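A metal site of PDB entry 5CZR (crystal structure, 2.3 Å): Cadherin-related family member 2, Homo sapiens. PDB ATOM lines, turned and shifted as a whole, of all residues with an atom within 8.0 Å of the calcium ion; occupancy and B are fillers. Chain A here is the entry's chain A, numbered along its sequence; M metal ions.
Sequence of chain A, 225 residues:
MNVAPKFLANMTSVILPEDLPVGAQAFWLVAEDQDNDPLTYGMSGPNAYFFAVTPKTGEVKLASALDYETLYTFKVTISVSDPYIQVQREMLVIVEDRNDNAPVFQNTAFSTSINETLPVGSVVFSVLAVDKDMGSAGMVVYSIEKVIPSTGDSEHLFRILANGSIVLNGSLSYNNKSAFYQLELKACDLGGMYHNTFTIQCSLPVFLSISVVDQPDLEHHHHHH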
ATOM      1  N   ASN A   2      14.943  24.386   8.786  1.00  0.00           N
ATOM      2  CA  ASN A   2      16.188  24.704   8.008  1.00  0.00           C
ATOM      3  C   ASN A   2      16.126  24.370   6.526  1.00  0.00           C
ATOM      4  O   ASN A   2      15.687  23.282   6.145  1.00  0.00           O
ATOM      5  CB  ASN A   2      17.463  24.028   8.579  1.00  0.00           C
ATOM      6  CG  ASN A   2      18.739  24.458   7.799  1.00  0.00           C
ATOM      7  OD1 ASN A   2      19.048  25.645   7.702  1.00  0.00           O
ATOM      8  ND2 ASN A   2      19.467  23.487   7.239  1.00  0.00           N
ATOM      9  N   VAL A   3      16.625  25.275   5.686  1.00  0.00           N
ATOM     10  CA  VAL A   3      16.849  25.013   4.272  1.00  0.00           C
ATOM     11  C   VAL A   3      18.350  24.682   3.994  1.00  0.00           C
ATOM     12  O   VAL A   3      19.256  25.368   4.489  1.00  0.00           O
ATOM     13  CB  VAL A   3      16.416  26.230   3.421  1.00  0.00           C
ATOM     14  CG1 VAL A   3      16.558  25.919   1.937  1.00  0.00           C
ATOM     15  CG2 VAL A   3      14.965  26.580   3.747  1.00  0.00           C
ATOM     16  N   ALA A   4      18.568  23.613   3.245  1.00  0.00           N
ATOM     17  CA  ALA A   4      19.915  23.196   2.888  1.00  0.00           C
ATOM     18  C   ALA A   4      20.566  24.244   1.988  1.00  0.00           C
ATOM     19  O   ALA A   4      19.880  24.823   1.146  1.00  0.00           O
ATOM     20  CB  ALA A   4      19.902  21.851   2.191  1.00  0.00           C
ATOM     21  N   PRO A   5      21.867  24.490   2.174  1.00  0.00           N
ATOM     22  CA  PRO A   5      22.582  25.337   1.211  1.00  0.00           C
ATOM     23  C   PRO A   5      22.697  24.641  -0.147  1.00  0.00           C
ATOM     24  O   PRO A   5      22.562  23.415  -0.234  1.00  0.00           O
ATOM     25  CB  PRO A   5      23.956  25.511   1.838  1.00  0.00           C
ATOM     26  CG  PRO A   5      24.116  24.285   2.687  1.00  0.00           C
ATOM     27  CD  PRO A   5      22.757  23.989   3.230  1.00  0.00           C
ATOM     28  N   LYS A   6      22.976  25.434  -1.165  1.00  0.00           N
ATOM     29  CA  LYS A   6      22.963  24.994  -2.549  1.00  0.00           C
ATOM     30  C   LYS A   6      24.095  25.712  -3.275  1.00  0.00           C
ATOM     31  O   LYS A   6      24.237  26.927  -3.183  1.00  0.00           O
ATOM     32  CB  LYS A   6      21.614  25.353  -3.188  1.00  0.00           C
ATOM     33  CG  LYS A   6      21.396  24.781  -4.588  1.00  0.00           C
ATOM     34  CD  LYS A   6      19.956  24.272  -4.800  1.00  0.00           C
ATOM     35  CE  LYS A   6      18.887  25.358  -4.678  1.00  0.00           C
ATOM     36  NZ  LYS A   6      18.794  26.184  -5.935  1.00  0.00           N
ATOM     37  N   GLU A  32      24.862  29.370  -1.760  1.00  0.00           N
ATOM     38  CA  GLU A  32      23.930  30.296  -1.102  1.00  0.00           C
ATOM     39  C   GLU A  32      23.031  29.509  -0.190  1.00  0.00           C
ATOM     40  O   GLU A  32      22.852  28.286  -0.327  1.00  0.00           O
ATOM     41  CB  GLU A  32      23.100  31.040  -2.137  1.00  0.00           C
ATOM     42  CG  GLU A  32      22.099  30.154  -2.883  1.00  0.00           C
ATOM     43  CD  GLU A  32      21.524  30.789  -4.163  1.00  0.00           C
ATOM     44  OE1 GLU A  32      22.192  31.680  -4.774  1.00  0.00           O
ATOM     45  OE2 GLU A  32      20.408  30.374  -4.579  1.00  0.00           O
ATOM     46  N   ASP A  33      22.468  30.229   0.775  1.00  0.00           N
ATOM     47  CA  ASP A  33      21.629  29.589   1.788  1.00  0.00           C
ATOM     48  C   ASP A  33      20.461  30.502   2.095  1.00  0.00           C
ATOM     49  O   ASP A  33      20.658  31.640   2.539  1.00  0.00           O
ATOM     50  CB  ASP A  33      22.444  29.322   3.067  1.00  0.00           C
ATOM     51  CG  ASP A  33      21.676  28.454   4.091  1.00  0.00           C
ATOM     52  OD1 ASP A  33      20.791  28.984   4.793  1.00  0.00           O
ATOM     53  OD2 ASP A  33      22.002  27.258   4.220  1.00  0.00           O
ATOM     54  N   GLN A  34      19.257  29.983   1.879  1.00  0.00           N
ATOM     55  CA  GLN A  34      17.999  30.755   2.066  1.00  0.00           C
ATOM     56  C   GLN A  34      17.803  31.291   3.502  1.00  0.00           C
ATOM     57  O   GLN A  34      17.126  32.279   3.673  1.00  0.00           O
ATOM     58  CB  GLN A  34      16.779  29.884   1.694  1.00  0.00           C
ATOM     59  CG  GLN A  34      15.632  30.646   0.984  1.00  0.00           C
ATOM     60  CD  GLN A  34      15.845  30.811  -0.526  1.00  0.00           C
ATOM     61  OE1 GLN A  34      16.821  30.315  -1.103  1.00  0.00           O
ATOM     62  NE2 GLN A  34      14.907  31.515  -1.156  1.00  0.00           N
ATOM     63  N   ASP A  35      18.399  30.650   4.496  1.00  0.00           N
ATOM     64  CA  ASP A  35      18.333  31.144   5.879  1.00  0.00           C
ATOM     65  C   ASP A  35      19.452  32.112   6.193  1.00  0.00           C
ATOM     66  O   ASP A  35      19.525  32.658   7.275  1.00  0.00           O
ATOM     67  CB  ASP A  35      18.411  29.998   6.878  1.00  0.00           C
ATOM     68  CG  ASP A  35      17.487  28.849   6.505  1.00  0.00           C
ATOM     69  OD1 ASP A  35      16.245  29.021   6.520  1.00  0.00           O
ATOM     70  OD2 ASP A  35      18.022  27.758   6.216  1.00  0.00           O
ATOM     71  N   ASN A  36      20.350  32.320   5.231  1.00  0.00           N
ATOM     72  CA  ASN A  36      21.502  33.175   5.439  1.00  0.00           C
ATOM     73  C   ASN A  36      22.478  32.645   6.503  1.00  0.00           C
ATOM     74  O   ASN A  36      23.130  33.409   7.213  1.00  0.00           O
ATOM     75  CB  ASN A  36      20.994  34.568   5.793  1.00  0.00           C
ATOM     76  CG  ASN A  36      21.708  35.651   5.046  1.00  0.00           C
ATOM     77  OD1 ASN A  36      21.719  35.703   3.793  1.00  0.00           O
ATOM     78  ND2 ASN A  36      22.316  36.545   5.809  1.00  0.00           N
ATOM     79  N   ASP A  37      22.586  31.311   6.599  1.00  0.00           N
ATOM     80  CA  ASP A  37      23.461  30.665   7.578  1.00  0.00           C
ATOM     81  C   ASP A  37      24.916  30.868   7.150  1.00  0.00           C
ATOM     82  O   ASP A  37      25.206  30.930   5.980  1.00  0.00           O
ATOM     83  CB  ASP A  37      23.194  29.152   7.655  1.00  0.00           C
ATOM     84  CG  ASP A  37      21.876  28.820   8.327  1.00  0.00           C
ATOM     85  OD1 ASP A  37      21.611  29.426   9.395  1.00  0.00           O
ATOM     86  OD2 ASP A  37      21.117  27.954   7.832  1.00  0.00           O
ATOM     87  N   PRO A  38      25.834  30.928   8.129  1.00  0.00           N
ATOM     88  CA  PRO A  38      27.247  30.849   7.795  1.00  0.00           C
ATOM     89  C   PRO A  38      27.537  29.478   7.207  1.00  0.00           C
ATOM     90  O   PRO A  38      27.017  28.479   7.704  1.00  0.00           O
ATOM     91  CB  PRO A  38      27.933  30.992   9.136  1.00  0.00           C
ATOM     92  CG  PRO A  38      26.959  30.475  10.120  1.00  0.00           C
ATOM     93  CD  PRO A  38      25.625  30.934   9.585  1.00  0.00           C
ATOM     94  N   LEU A  39      28.352  29.457   6.139  1.00  0.00           N
ATOM     95  CA  LEU A  39      28.609  28.246   5.334  1.00  0.00           C
ATOM     96  C   LEU A  39      30.068  27.910   5.353  1.00  0.00           C
ATOM     97  O   LEU A  39      30.923  28.804   5.324  1.00  0.00           O
ATOM     98  CB  LEU A  39      28.201  28.486   3.880  1.00  0.00           C
ATOM     99  CG  LEU A  39      26.733  28.907   3.671  1.00  0.00           C
ATOM    100  CD1 LEU A  39      26.414  29.027   2.196  1.00  0.00           C
ATOM    101  CD2 LEU A  39      25.791  27.913   4.360  1.00  0.00           C
ATOM    102  N   SER A  81      28.478  23.211   3.876  1.00  0.00           N
ATOM    103  CA  SER A  81      27.758  22.875   5.084  1.00  0.00           C
ATOM    104  C   SER A  81      27.225  24.146   5.729  1.00  0.00           C
ATOM    105  O   SER A  81      27.978  25.107   5.898  1.00  0.00           O
ATOM    106  CB  SER A  81      28.690  22.176   6.057  1.00  0.00           C
ATOM    107  OG  SER A  81      29.108  20.949   5.532  1.00  0.00           O
ATOM    108  N   ASP A  82      25.936  24.182   6.060  1.00  0.00           N
ATOM    109  CA  ASP A  82      25.468  25.197   7.030  1.00  0.00           C
ATOM    110  C   ASP A  82      25.698  24.563   8.426  1.00  0.00           C
ATOM    111  O   ASP A  82      26.420  23.558   8.527  1.00  0.00           O
ATOM    112  CB  ASP A  82      24.054  25.694   6.693  1.00  0.00           C
ATOM    113  CG  ASP A  82      22.963  24.657   6.921  1.00  0.00           C
ATOM    114  OD1 ASP A  82      23.214  23.587   7.538  1.00  0.00           O
ATOM    115  OD2 ASP A  82      21.849  24.914   6.476  1.00  0.00           O
ATOM    116  N   PRO A  83      25.175  25.176   9.503  1.00  0.00           N
ATOM    117  CA  PRO A  83      25.411  24.575  10.843  1.00  0.00           C
ATOM    118  C   PRO A  83      24.730  23.223  11.054  1.00  0.00           C
ATOM    119  O   PRO A  83      25.167  22.458  11.910  1.00  0.00           O
ATOM    120  CB  PRO A  83      24.832  25.606  11.794  1.00  0.00           C
ATOM    121  CG  PRO A  83      24.875  26.898  11.047  1.00  0.00           C
ATOM    122  CD  PRO A  83      24.606  26.523   9.614  1.00  0.00           C
ATOM    123  N   TYR A  84      23.733  22.890  10.206  1.00  0.00           N
ATOM    124  CA  TYR A  84      22.848  21.738  10.407  1.00  0.00           C
ATOM    125  C   TYR A  84      23.014  20.581   9.426  1.00  0.00           C
ATOM    126  O   TYR A  84      22.747  19.444   9.767  1.00  0.00           O
ATOM    127  CB  TYR A  84      21.396  22.214  10.363  1.00  0.00           C
ATOM    128  CG  TYR A  84      21.212  23.522  11.081  1.00  0.00           C
ATOM    129  CD1 TYR A  84      21.189  23.576  12.475  1.00  0.00           C
ATOM    130  CD2 TYR A  84      21.082  24.706  10.368  1.00  0.00           C
ATOM    131  CE1 TYR A  84      21.035  24.782  13.140  1.00  0.00           C
ATOM    132  CE2 TYR A  84      20.907  25.913  11.025  1.00  0.00           C
ATOM    133  CZ  TYR A  84      20.916  25.938  12.405  1.00  0.00           C
ATOM    134  OH  TYR A  84      20.770  27.143  13.033  1.00  0.00           O
ATOM    135  N   ILE A  85      23.406  20.872   8.179  1.00  0.00           N
ATOM    136  CA  ILE A  85      23.490  19.837   7.170  1.00  0.00           C
ATOM    137  C   ILE A  85      24.695  20.012   6.249  1.00  0.00           C
ATOM    138  O   ILE A  85      25.054  21.149   5.886  1.00  0.00           O
ATOM    139  CB  ILE A  85      22.159  19.742   6.380  1.00  0.00           C
ATOM    140  CG1 ILE A  85      22.144  18.469   5.510  1.00  0.00           C
ATOM    141  CG2 ILE A  85      21.874  21.031   5.582  1.00  0.00           C
ATOM    142  CD1 ILE A  85      20.801  18.158   4.850  1.00  0.00           C
HETATM  143 CA    CA M   1      20.335  26.802   6.078  1.00  0.00          CA
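N of Tyr 84 sits at hydrogen-bond distance from OD1 of Asp 82, at 2.8 Å. N of Ile 85 lies within hydrogen-bond range of OD1 of Asp 82, at 2.8 Å. OD1 of Asp 33 lies close to N of Asn 36 (3.4 Å).
Of the 18 residues printed, 6 come within 4 Å of the calcium ion.
The calcium ion is bound by OD2 of Asp 37 (2.2 Å), OD1 of Asn 2 (2.4 Å), O of Val 3 (2.4 Å), OD2 of Asp 82 (2.5 Å), OD2 of Asp 35 (2.5 Å), OD2 of Asp 33 (2.5 Å) and OD1 of Asp 33 (2.6 Å). The calcium ion has seven donor atoms within binding distance.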
